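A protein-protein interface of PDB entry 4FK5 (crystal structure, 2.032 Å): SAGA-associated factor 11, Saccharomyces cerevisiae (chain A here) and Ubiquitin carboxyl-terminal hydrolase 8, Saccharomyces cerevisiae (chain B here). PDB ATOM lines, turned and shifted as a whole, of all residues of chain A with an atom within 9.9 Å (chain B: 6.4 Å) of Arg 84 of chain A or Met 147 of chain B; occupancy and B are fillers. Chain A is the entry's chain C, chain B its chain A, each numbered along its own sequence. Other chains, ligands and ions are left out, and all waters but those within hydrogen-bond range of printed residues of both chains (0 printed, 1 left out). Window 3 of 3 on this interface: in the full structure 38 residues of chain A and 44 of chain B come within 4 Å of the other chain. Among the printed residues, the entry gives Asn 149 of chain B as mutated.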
ATOM      1  N   GLN A  64       9.478  29.269  13.462  1.00  0.00           N
ATOM      2  CA  GLN A  64       9.371  29.440  12.015  1.00  0.00           C
ATOM      3  C   GLN A  64       8.085  30.224  11.705  1.00  0.00           C
ATOM      4  O   GLN A  64       7.088  30.107  12.443  1.00  0.00           O
ATOM      5  CB  GLN A  64       9.351  28.041  11.318  1.00  0.00           C
ATOM      6  CG  GLN A  64       8.598  26.972  12.125  1.00  0.00           C
ATOM      7  CD  GLN A  64       8.469  25.639  11.412  1.00  0.00           C
ATOM      8  OE1 GLN A  64       7.354  25.119  11.234  1.00  0.00           O
ATOM      9  NE2 GLN A  64       9.606  25.063  11.011  1.00  0.00           N
ATOM     10  N   GLU A  66       4.904  30.373   9.981  1.00  0.00           N
ATOM     11  CA  GLU A  66       4.172  29.212   9.480  1.00  0.00           C
ATOM     12  C   GLU A  66       3.443  29.577   8.147  1.00  0.00           C
ATOM     13  O   GLU A  66       3.117  28.703   7.345  1.00  0.00           O
ATOM     14  CB  GLU A  66       3.188  28.644  10.580  1.00  0.00           C
ATOM     15  CG  GLU A  66       3.912  27.805  11.706  1.00  0.00           C
ATOM     16  CD  GLU A  66       2.962  27.191  12.802  1.00  0.00           C
ATOM     17  OE1 GLU A  66       1.725  27.385  12.770  1.00  0.00           O
ATOM     18  OE2 GLU A  66       3.479  26.510  13.704  1.00  0.00           O
ATOM     19  N   SER A  67       3.313  30.871   7.887  1.00  0.00           N
ATOM     20  CA  SER A  67       2.644  31.357   6.678  1.00  0.00           C
ATOM     21  C   SER A  67       3.570  31.379   5.459  1.00  0.00           C
ATOM     22  O   SER A  67       3.092  31.479   4.328  1.00  0.00           O
ATOM     23  CB  SER A  67       2.098  32.755   6.910  1.00  0.00           C
ATOM     24  OG  SER A  67       3.156  33.662   7.093  1.00  0.00           O
ATOM     25  N   SER A  68       4.886  31.244   5.676  1.00  0.00           N
ATOM     26  CA  SER A  68       5.810  31.089   4.550  1.00  0.00           C
ATOM     27  C   SER A  68       6.057  29.613   4.189  1.00  0.00           C
ATOM     28  O   SER A  68       6.728  29.326   3.246  1.00  0.00           O
ATOM     29  CB  SER A  68       7.106  31.787   4.842  1.00  0.00           C
ATOM     30  OG  SER A  68       7.605  31.360   6.084  1.00  0.00           O
ATOM     31  N   GLN A  69       5.427  28.692   4.909  1.00  0.00           N
ATOM     32  CA  GLN A  69       5.513  27.285   4.587  1.00  0.00           C
ATOM     33  C   GLN A  69       4.293  26.861   3.757  1.00  0.00           C
ATOM     34  O   GLN A  69       3.256  27.503   3.788  1.00  0.00           O
ATOM     35  CB  GLN A  69       5.548  26.456   5.857  1.00  0.00           C
ATOM     36  CG  GLN A  69       6.650  26.841   6.849  1.00  0.00           C
ATOM     37  CD  GLN A  69       6.519  26.064   8.160  1.00  0.00           C
ATOM     38  OE1 GLN A  69       5.930  26.550   9.129  1.00  0.00           O
ATOM     39  NE2 GLN A  69       6.979  24.813   8.154  1.00  0.00           N
ATOM     40  N   TYR A  70       4.446  25.793   3.024  1.00  0.00           N
ATOM     41  CA  TYR A  70       3.371  25.242   2.263  1.00  0.00           C
ATOM     42  C   TYR A  70       3.355  23.759   2.406  1.00  0.00           C
ATOM     43  O   TYR A  70       4.386  23.151   2.665  1.00  0.00           O
ATOM     44  CB  TYR A  70       3.514  25.637   0.787  1.00  0.00           C
ATOM     45  CG  TYR A  70       4.705  25.014   0.099  1.00  0.00           C
ATOM     46  CD1 TYR A  70       4.609  23.783  -0.526  1.00  0.00           C
ATOM     47  CD2 TYR A  70       5.938  25.675   0.068  1.00  0.00           C
ATOM     48  CE1 TYR A  70       5.719  23.217  -1.176  1.00  0.00           C
ATOM     49  CE2 TYR A  70       7.045  25.112  -0.551  1.00  0.00           C
ATOM     50  CZ  TYR A  70       6.937  23.909  -1.169  1.00  0.00           C
ATOM     51  OH  TYR A  70       8.042  23.369  -1.767  1.00  0.00           O
ATOM     52  N   ILE A  71       2.186  23.175   2.137  1.00  0.00           N
ATOM     53  CA  ILE A  71       1.952  21.720   2.144  1.00  0.00           C
ATOM     54  C   ILE A  71       1.368  21.372   0.824  1.00  0.00           C
ATOM     55  O   ILE A  71       0.511  22.074   0.355  1.00  0.00           O
ATOM     56  CB  ILE A  71       0.857  21.308   3.201  1.00  0.00           C
ATOM     57  CG1 ILE A  71       1.144  21.888   4.560  1.00  0.00           C
ATOM     58  CG2 ILE A  71       0.650  19.786   3.240  1.00  0.00           C
ATOM     59  CD1 ILE A  71       2.267  21.267   5.265  1.00  0.00           C
ATOM     60  N   HIS A  72       1.756  20.245   0.265  1.00  0.00           N
ATOM     61  CA  HIS A  72       1.157  19.734  -0.966  1.00  0.00           C
ATOM     62  C   HIS A  72      -0.149  19.028  -0.670  1.00  0.00           C
ATOM     63  O   HIS A  72      -0.182  18.132   0.134  1.00  0.00           O
ATOM     64  CB  HIS A  72       2.141  18.770  -1.645  1.00  0.00           C
ATOM     65  CG  HIS A  72       1.778  18.427  -3.058  1.00  0.00           C
ATOM     66  ND1 HIS A  72       1.961  19.298  -4.095  1.00  0.00           N
ATOM     67  CD2 HIS A  72       1.210  17.294  -3.593  1.00  0.00           C
ATOM     68  CE1 HIS A  72       1.521  18.732  -5.219  1.00  0.00           C
ATOM     69  NE2 HIS A  72       1.074  17.498  -4.918  1.00  0.00           N
ATOM     70  N   CYS A  73      -1.250  19.456  -1.286  1.00  0.00           N
ATOM     71  CA  CYS A  73      -2.542  18.825  -1.032  1.00  0.00           C
ATOM     72  C   CYS A  73      -2.665  17.649  -1.940  1.00  0.00           C
ATOM     73  O   CYS A  73      -2.564  17.784  -3.140  1.00  0.00           O
ATOM     74  CB  CYS A  73      -3.704  19.784  -1.260  1.00  0.00           C
ATOM     75  SG  CYS A  73      -5.372  19.015  -1.017  1.00  0.00           S
ATOM     76  N   ARG A  78      -2.193  20.675  -5.539  1.00  0.00           N
ATOM     77  CA  ARG A  78      -1.597  22.024  -5.380  1.00  0.00           C
ATOM     78  C   ARG A  78      -0.787  22.144  -4.108  1.00  0.00           C
ATOM     79  O   ARG A  78      -1.088  21.472  -3.083  1.00  0.00           O
ATOM     80  CB  ARG A  78      -2.681  23.119  -5.308  1.00  0.00           C
ATOM     81  CG  ARG A  78      -3.624  23.178  -6.505  1.00  0.00           C
ATOM     82  CD  ARG A  78      -4.868  24.037  -6.199  1.00  0.00           C
ATOM     83  NE  ARG A  78      -4.751  25.383  -6.771  1.00  0.00           N
ATOM     84  CZ  ARG A  78      -4.192  26.432  -6.157  1.00  0.00           C
ATOM     85  NH1 ARG A  78      -3.709  26.321  -4.910  1.00  0.00           N
ATOM     86  NH2 ARG A  78      -4.143  27.607  -6.782  1.00  0.00           N
ATOM     87  N   ASP A  79       0.149  23.110  -4.122  1.00  0.00           N
ATOM     88  CA  ASP A  79       0.744  23.601  -2.931  1.00  0.00           C
ATOM     89  C   ASP A  79      -0.205  24.577  -2.307  1.00  0.00           C
ATOM     90  O   ASP A  79      -0.801  25.398  -2.982  1.00  0.00           O
ATOM     91  CB  ASP A  79       2.099  24.279  -3.216  1.00  0.00           C
ATOM     92  CG  ASP A  79       3.209  23.267  -3.669  1.00  0.00           C
ATOM     93  OD1 ASP A  79       3.029  22.049  -3.456  1.00  0.00           O
ATOM     94  OD2 ASP A  79       4.297  23.727  -4.200  1.00  0.00           O
ATOM     95  N   VAL A  80      -0.357  24.479  -0.988  1.00  0.00           N
ATOM     96  CA  VAL A  80      -1.272  25.353  -0.217  1.00  0.00           C
ATOM     97  C   VAL A  80      -0.483  25.950   0.919  1.00  0.00           C
ATOM     98  O   VAL A  80       0.191  25.227   1.644  1.00  0.00           O
ATOM     99  CB  VAL A  80      -2.437  24.460   0.359  1.00  0.00           C
ATOM    100  CG1 VAL A  80      -3.273  25.221   1.360  1.00  0.00           C
ATOM    101  CG2 VAL A  80      -3.281  23.892  -0.813  1.00  0.00           C
ATOM    102  N   SER A  81      -0.613  27.236   1.167  1.00  0.00           N
ATOM    103  CA  SER A  81       0.053  27.801   2.316  1.00  0.00           C
ATOM    104  C   SER A  81      -0.442  27.078   3.601  1.00  0.00           C
ATOM    105  O   SER A  81      -1.655  26.807   3.774  1.00  0.00           O
ATOM    106  CB  SER A  81      -0.147  29.315   2.375  1.00  0.00           C
ATOM    107  OG  SER A  81       0.369  29.897   1.139  1.00  0.00           O
ATOM    108  N   ALA A  82       0.514  26.702   4.451  1.00  0.00           N
ATOM    109  CA  ALA A  82       0.250  25.779   5.565  1.00  0.00           C
ATOM    110  C   ALA A  82      -0.823  26.325   6.504  1.00  0.00           C
ATOM    111  O   ALA A  82      -1.706  25.578   6.965  1.00  0.00           O
ATOM    112  CB  ALA A  82       1.562  25.506   6.357  1.00  0.00           C
ATOM    113  N   ASN A  83      -0.811  27.638   6.742  1.00  0.00           N
ATOM    114  CA  ASN A  83      -1.797  28.243   7.634  1.00  0.00           C
ATOM    115  C   ASN A  83      -3.207  28.354   6.994  1.00  0.00           C
ATOM    116  O   ASN A  83      -4.161  28.852   7.638  1.00  0.00           O
ATOM    117  CB  ASN A  83      -1.328  29.595   8.114  1.00  0.00           C
ATOM    118  CG  ASN A  83      -1.309  30.635   7.002  1.00  0.00           C
ATOM    119  OD1 ASN A  83      -1.039  30.327   5.821  1.00  0.00           O
ATOM    120  ND2 ASN A  83      -1.599  31.821   7.348  1.00  0.00           N
ATOM    121  N   ARG A  84      -3.356  27.827   5.770  1.00  0.00           N
ATOM    122  CA  ARG A  84      -4.644  27.840   5.087  1.00  0.00           C
ATOM    123  C   ARG A  84      -5.169  26.480   4.822  1.00  0.00           C
ATOM    124  O   ARG A  84      -6.147  26.343   4.098  1.00  0.00           O
ATOM    125  CB  ARG A  84      -4.545  28.585   3.741  1.00  0.00           C
ATOM    126  CG  ARG A  84      -4.401  30.066   3.895  1.00  0.00           C
ATOM    127  CD  ARG A  84      -5.760  30.720   4.201  1.00  0.00           C
ATOM    128  NE  ARG A  84      -6.693  30.559   3.075  1.00  0.00           N
ATOM    129  CZ  ARG A  84      -7.905  31.115   3.012  1.00  0.00           C
ATOM    130  NH1 ARG A  84      -8.335  31.867   3.994  1.00  0.00           N
ATOM    131  NH2 ARG A  84      -8.674  30.931   1.945  1.00  0.00           N
ATOM    132  N   LEU A  85      -4.468  25.450   5.276  1.00  0.00           N
ATOM    133  CA  LEU A  85      -4.795  24.119   4.829  1.00  0.00           C
ATOM    134  C   LEU A  85      -6.207  23.714   5.276  1.00  0.00           C
ATOM    135  O   LEU A  85      -6.884  23.073   4.543  1.00  0.00           O
ATOM    136  CB  LEU A  85      -3.800  23.075   5.330  1.00  0.00           C
ATOM    137  CG  LEU A  85      -3.348  21.949   4.430  1.00  0.00           C
ATOM    138  CD1 LEU A  85      -3.140  20.716   5.233  1.00  0.00           C
ATOM    139  CD2 LEU A  85      -4.252  21.693   3.266  1.00  0.00           C
ATOM    140  N   ALA A  86      -6.609  24.068   6.497  1.00  0.00           N
ATOM    141  CA  ALA A  86      -7.938  23.637   7.017  1.00  0.00           C
ATOM    142  C   ALA A  86      -9.080  24.314   6.251  1.00  0.00           C
ATOM    143  O   ALA A  86     -10.027  23.661   5.860  1.00  0.00           O
ATOM    144  CB  ALA A  86      -8.050  23.909   8.515  1.00  0.00           C
ATOM    145  N   ALA A  87      -8.934  25.599   5.939  1.00  0.00           N
ATOM    146  CA  ALA A  87      -9.905  26.278   5.039  1.00  0.00           C
ATOM    147  C   ALA A  87      -9.869  25.658   3.638  1.00  0.00           C
ATOM    148  O   ALA A  87     -10.913  25.384   3.003  1.00  0.00           O
ATOM    149  CB  ALA A  87      -9.597  27.784   4.962  1.00  0.00           C
ATOM    150  N   HIS A  88      -8.673  25.399   3.153  1.00  0.00           N
ATOM    151  CA  HIS A  88      -8.532  24.799   1.838  1.00  0.00           C
ATOM    152  C   HIS A  88      -9.252  23.490   1.742  1.00  0.00           C
ATOM    153  O   HIS A  88      -9.975  23.212   0.771  1.00  0.00           O
ATOM    154  CB  HIS A  88      -7.047  24.618   1.471  1.00  0.00           C
ATOM    155  CG  HIS A  88      -6.837  23.871   0.197  1.00  0.00           C
ATOM    156  ND1 HIS A  88      -6.930  24.467  -1.010  1.00  0.00           N
ATOM    157  CD2 HIS A  88      -6.611  22.523  -0.036  1.00  0.00           C
ATOM    158  CE1 HIS A  88      -6.776  23.526  -1.989  1.00  0.00           C
ATOM    159  NE2 HIS A  88      -6.565  22.335  -1.382  1.00  0.00           N
ATOM    160  N   LEU A  89      -9.024  22.640   2.713  1.00  0.00           N
ATOM    161  CA  LEU A  89      -9.671  21.309   2.733  1.00  0.00           C
ATOM    162  C   LEU A  89     -11.244  21.402   2.675  1.00  0.00           C
ATOM    163  O   LEU A  89     -11.880  20.684   1.909  1.00  0.00           O
ATOM    164  CB  LEU A  89      -9.204  20.517   3.973  1.00  0.00           C
ATOM    165  CG  LEU A  89      -7.754  19.972   3.894  1.00  0.00           C
ATOM    166  CD1 LEU A  89      -7.349  19.243   5.183  1.00  0.00           C
ATOM    167  CD2 LEU A  89      -7.595  19.065   2.729  1.00  0.00           C
ATOM    168  N   GLN A  90     -11.832  22.310   3.450  1.00  0.00           N
ATOM    169  CA  GLN A  90     -13.301  22.579   3.391  1.00  0.00           C
ATOM    170  C   GLN A  90     -13.785  22.721   1.992  1.00  0.00           C
ATOM    171  O   GLN A  90     -14.788  22.144   1.625  1.00  0.00           O
ATOM    172  CB  GLN A  90     -13.675  23.854   4.173  1.00  0.00           C
ATOM    173  CG  GLN A  90     -13.540  23.740   5.702  1.00  0.00           C
ATOM    174  CD  GLN A  90     -14.679  22.937   6.346  1.00  0.00           C
ATOM    175  OE1 GLN A  90     -14.607  22.565   7.546  1.00  0.00           O
ATOM    176  NE2 GLN A  90     -15.747  22.677   5.563  1.00  0.00           N
ATOM    177  N   ARG A  91     -13.043  23.475   1.188  1.00  0.00           N
ATOM    178  CA  ARG A  91     -13.398  23.745  -0.188  1.00  0.00           C
ATOM    179  C   ARG A  91     -12.946  22.685  -1.111  1.00  0.00           C
ATOM    180  O   ARG A  91     -13.537  22.494  -2.150  1.00  0.00           O
ATOM    181  CB  ARG A  91     -12.795  25.089  -0.661  1.00  0.00           C
ATOM    182  CG  ARG A  91     -13.734  26.256  -0.506  1.00  0.00           C
ATOM    183  CD  ARG A  91     -13.070  27.591  -0.797  1.00  0.00           C
ATOM    184  NE  ARG A  91     -12.239  28.057   0.330  1.00  0.00           N
ATOM    185  CZ  ARG A  91     -10.901  27.997   0.356  1.00  0.00           C
ATOM    186  NH1 ARG A  91     -10.249  27.504  -0.656  1.00  0.00           N
ATOM    187  NH2 ARG A  91     -10.232  28.450   1.394  1.00  0.00           N
ATOM    188  N   CYS A  92     -11.852  22.028  -0.801  1.00  0.00           N
ATOM    189  CA  CYS A  92     -11.253  21.083  -1.775  1.00  0.00           C
ATOM    190  C   CYS A  92     -11.839  19.675  -1.683  1.00  0.00           C
ATOM    191  O   CYS A  92     -11.958  18.993  -2.686  1.00  0.00           O
ATOM    192  CB  CYS A  92      -9.739  20.995  -1.564  1.00  0.00           C
ATOM    193  SG  CYS A  92      -8.915  19.894  -2.697  1.00  0.00           S
ATOM    194  N   LEU B 144       2.797  20.750  15.900  1.00  0.00           N
ATOM    195  CA  LEU B 144       1.742  20.699  14.888  1.00  0.00           C
ATOM    196  C   LEU B 144       1.392  22.111  14.404  1.00  0.00           C
ATOM    197  O   LEU B 144       0.994  22.989  15.212  1.00  0.00           O
ATOM    198  CB  LEU B 144       0.503  20.024  15.441  1.00  0.00           C
ATOM    199  CG  LEU B 144       0.640  18.544  15.794  1.00  0.00           C
ATOM    200  CD1 LEU B 144      -0.571  18.083  16.613  1.00  0.00           C
ATOM    201  CD2 LEU B 144       0.799  17.688  14.534  1.00  0.00           C
ATOM    202  N   ILE B 145       1.573  22.339  13.103  1.00  0.00           N
ATOM    203  CA  ILE B 145       1.357  23.629  12.519  1.00  0.00           C
ATOM    204  C   ILE B 145      -0.055  24.028  12.719  1.00  0.00           C
ATOM    205  O   ILE B 145      -0.946  23.201  12.586  1.00  0.00           O
ATOM    206  CB  ILE B 145       1.691  23.631  10.985  1.00  0.00           C
ATOM    207  CG1 ILE B 145       3.166  23.427  10.771  1.00  0.00           C
ATOM    208  CG2 ILE B 145       1.330  24.985  10.336  1.00  0.00           C
ATOM    209  CD1 ILE B 145       3.542  23.436   9.277  1.00  0.00           C
ATOM    210  N   ASN B 146      -0.292  25.309  12.989  1.00  0.00           N
ATOM    211  CA  ASN B 146      -1.684  25.844  12.982  1.00  0.00           C
ATOM    212  C   ASN B 146      -2.220  26.021  11.530  1.00  0.00           C
ATOM    213  O   ASN B 146      -1.753  26.861  10.790  1.00  0.00           O
ATOM    214  CB  ASN B 146      -1.768  27.186  13.702  1.00  0.00           C
ATOM    215  CG  ASN B 146      -3.217  27.675  13.899  1.00  0.00           C
ATOM    216  OD1 ASN B 146      -4.162  27.220  13.222  1.00  0.00           O
ATOM    217  ND2 ASN B 146      -3.404  28.573  14.886  1.00  0.00           N
ATOM    218  N   MET B 147      -3.251  25.295  11.177  1.00  0.00           N
ATOM    219  CA  MET B 147      -3.611  25.183   9.765  1.00  0.00           C
ATOM    220  C   MET B 147      -4.917  25.874   9.295  1.00  0.00           C
ATOM    221  O   MET B 147      -5.246  25.789   8.146  1.00  0.00           O
ATOM    222  CB  MET B 147      -3.705  23.726   9.420  1.00  0.00           C
ATOM    223  CG  MET B 147      -2.351  23.014   9.246  1.00  0.00           C
ATOM    224  SD  MET B 147      -2.637  21.304   8.810  1.00  0.00           S
ATOM    225  CE  MET B 147      -0.931  20.696   9.080  1.00  0.00           C
ATOM    226  N   GLY B 148      -5.746  26.415  10.158  1.00  0.00           N
ATOM    227  CA  GLY B 148      -5.611  27.627  10.859  1.00  0.00           C
ATOM    228  C   GLY B 148      -6.934  27.669  11.672  1.00  0.00           C
ATOM    229  O   GLY B 148      -7.944  27.009  11.304  1.00  0.00           O
ATOM    230  N   ASN B 149      -6.901  28.340  12.811  1.00  0.00           N
ATOM    231  CA  ASN B 149      -7.805  28.035  13.927  1.00  0.00           C
ATOM    232  C   ASN B 149      -7.884  26.510  14.239  1.00  0.00           C
ATOM    233  O   ASN B 149      -8.983  25.954  14.433  1.00  0.00           O
ATOM    234  CB  ASN B 149      -9.190  28.604  13.660  1.00  0.00           C
ATOM    235  CG  ASN B 149      -9.201  30.141  13.625  1.00  0.00           C
ATOM    236  OD1 ASN B 149     -10.137  30.750  13.091  1.00  0.00           O
ATOM    237  ND2 ASN B 149      -8.163  30.762  14.174  1.00  0.00           N
ATOM    238  N   THR B 150      -6.723  25.826  14.251  1.00  0.00           N
ATOM    239  CA  THR B 150      -6.717  24.394  14.598  1.00  0.00           C
ATOM    240  C   THR B 150      -5.981  24.108  15.936  1.00  0.00           C
ATOM    241  O   THR B 150      -5.848  22.958  16.326  1.00  0.00           O
ATOM    242  CB  THR B 150      -6.122  23.510  13.447  1.00  0.00           C
ATOM    243  OG1 THR B 150      -4.779  23.922  13.154  1.00  0.00           O
ATOM    244  CG2 THR B 150      -6.992  23.611  12.210  1.00  0.00           C
ATOM    245  N   CYS B 151      -5.553  25.139  16.635  1.00  0.00           N
ATOM    246  CA  CYS B 151      -4.893  24.932  17.914  1.00  0.00           C
ATOM    247  C   CYS B 151      -5.829  24.339  18.975  1.00  0.00           C
ATOM    248  O   CYS B 151      -5.367  23.723  19.887  1.00  0.00           O
ATOM    249  CB  CYS B 151      -4.206  26.206  18.423  1.00  0.00           C
ATOM    250  SG  CYS B 151      -5.311  27.603  18.719  1.00  0.00           S
ATOM    251  N   GLN B 218       3.584  16.353   9.685  1.00  0.00           N
ATOM    252  CA  GLN B 218       2.196  16.852   9.709  1.00  0.00           C
ATOM    253  C   GLN B 218       1.179  15.939   9.073  1.00  0.00           C
ATOM    254  O   GLN B 218      -0.018  16.227   9.103  1.00  0.00           O
ATOM    255  CB  GLN B 218       2.093  18.192   9.032  1.00  0.00           C
ATOM    256  CG  GLN B 218       3.087  19.220   9.513  1.00  0.00           C
ATOM    257  CD  GLN B 218       2.934  19.569  10.984  1.00  0.00           C
ATOM    258  OE1 GLN B 218       3.883  19.374  11.786  1.00  0.00           O
ATOM    259  NE2 GLN B 218       1.817  20.140  11.333  1.00  0.00           N
ATOM    260  N   PHE B 221      -1.732  14.466  11.152  1.00  0.00           N
ATOM    261  CA  PHE B 221      -2.643  15.547  11.535  1.00  0.00           C
ATOM    262  C   PHE B 221      -3.538  15.969  10.334  1.00  0.00           C
ATOM    263  O   PHE B 221      -4.755  16.203  10.484  1.00  0.00           O
ATOM    264  CB  PHE B 221      -1.848  16.734  12.072  1.00  0.00           C
ATOM    265  CG  PHE B 221      -2.704  17.876  12.591  1.00  0.00           C
ATOM    266  CD1 PHE B 221      -3.733  17.652  13.480  1.00  0.00           C
ATOM    267  CD2 PHE B 221      -2.429  19.188  12.212  1.00  0.00           C
ATOM    268  CE1 PHE B 221      -4.494  18.700  13.979  1.00  0.00           C
ATOM    269  CE2 PHE B 221      -3.201  20.244  12.700  1.00  0.00           C
ATOM    270  CZ  PHE B 221      -4.243  19.994  13.570  1.00  0.00           C
ATOM    271  N   ILE B 222      -2.955  16.019   9.152  1.00  0.00           N
ATOM    272  CA  ILE B 222      -3.732  16.326   7.954  1.00  0.00           C
ATOM    273  C   ILE B 222      -4.765  15.265   7.698  1.00  0.00           C
ATOM    274  O   ILE B 222      -5.892  15.576   7.355  1.00  0.00           O
ATOM    275  CB  ILE B 222      -2.827  16.521   6.744  1.00  0.00           C
ATOM    276  CG1 ILE B 222      -1.987  17.790   6.952  1.00  0.00           C
ATOM    277  CG2 ILE B 222      -3.655  16.617   5.434  1.00  0.00           C
ATOM    278  CD1 ILE B 222      -0.752  17.859   6.073  1.00  0.00           C
ATOM    279  N   LEU B 225      -7.685  15.864  10.069  1.00  0.00           N
ATOM    280  CA  LEU B 225      -8.524  16.949   9.584  1.00  0.00           C
ATOM    281  C   LEU B 225      -9.407  16.424   8.496  1.00  0.00           C
ATOM    282  O   LEU B 225     -10.591  16.773   8.410  1.00  0.00           O
ATOM    283  CB  LEU B 225      -7.672  18.110   9.029  1.00  0.00           C
ATOM    284  CG  LEU B 225      -6.940  19.006   9.987  1.00  0.00           C
ATOM    285  CD1 LEU B 225      -6.237  20.104   9.162  1.00  0.00           C
ATOM    286  CD2 LEU B 225      -7.904  19.605  11.012  1.00  0.00           C
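The backbone NH (N) of Asn 146 of chain B is in hydrogen-bond range of the side-chain carboxylate (OE1) of Glu 66 of chain A, at 2.9 Å.
N of Leu 85 of chain A sits at hydrogen-bond distance from O of Met 147 of chain B (3.0 Å).
The backbone carbonyl oxygen (O) of Met 147 of chain B is in hydrogen-bond range of the backbone NH (N) of Ala 86 of chain A (2.7 Å).
O of Asn 83 of chain A lies close to O of Met 147 of chain B (3.3 Å).
N of Ile 145 of chain B sits close to NE2 of Gln 218 of chain B.
The side-chain amide oxygen (OD1) of Asn 146 of chain B lies within hydrogen-bond range of the backbone NH (N) of Asn 149 of chain B, at 3.0 Å.
The side-chain amide oxygen (OD1) of Asn 146 of chain B is in hydrogen-bond range of the backbone NH (N) of Thr 150 of chain B.
N of Met 147 of chain B sits at hydrogen-bond distance from OG1 of Thr 150 of chain B (2.9 Å).
OE1 of Gln 64 of chain A lies close to OE1 of Gln 69 of chain A (2.9 Å).
The backbone carbonyl oxygen of Gln 69 of chain A sits at hydrogen-bond distance from the backbone NH of Ala 82 of chain A, 2.9 Å away.
Among the printed residues, merely in contact across the chains: Arg 84 of chain A with Met 147 of chain B, Ala 82 of chain A with Met 147 of chain B, Glu 66 of chain A with Ile 145 of chain B, Asn 83 of chain A with Asn 146 of chain B, Leu 85 of chain A with Ile 222 of chain B, Ile 71 of chain A with Ile 222 of chain B, Asn 83 of chain A with Gly 148 of chain B, Ala 86 of chain A with Gly 148 of chain B, Ala 86 of chain A with Thr 150 of chain B and Gln 69 of chain A with Ile 145 of chain B.
Gln 64 of chain A touches none of the printed residues of chain B.
Tyr 70 of chain A touches none of the printed residues of chain B.
Printed residues of chain B within 4 Å of Leu 85 of chain A: Met 147 (3.0 Å) and Ile 222 (3.6 Å).
Met 147 of chain B touches just these residues of chain A: Ala 82, Asn 83, Arg 84, Leu 85 and Ala 86.
Of the printed residues of chain A, Thr 150 of chain B touches Ala 86 (3.9 Å).
The nearest residue of chain B that does not touch Arg 84 of chain A is Gly 148 of chain B (5.2 Å).
Hydrophobic or aromatic side chains of chain B within 4 Å of the printed part of chain A: Ile 145, Met 147 and Ile 222.
Of the 24 printed residues of chain A, 8 touch a printed residue of chain B.
Printed residues of chain A that touch a printed residue of chain B: Glu 66, Gln 69, Ile 71, Ala 82, Asn 83, Arg 84, Leu 85 and Ala 86.
Hydrophobic or aromatic side chains of chain A within 4 Å of the printed part of chain B: Ile 71, Leu 85 and Ala 86.
Among the printed residues, 14 pairs touch across the chains.
Among the printed residues, no Asp or Glu carboxylate lies within 4 Å of a Lys or Arg side-chain nitrogen of the other chain.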
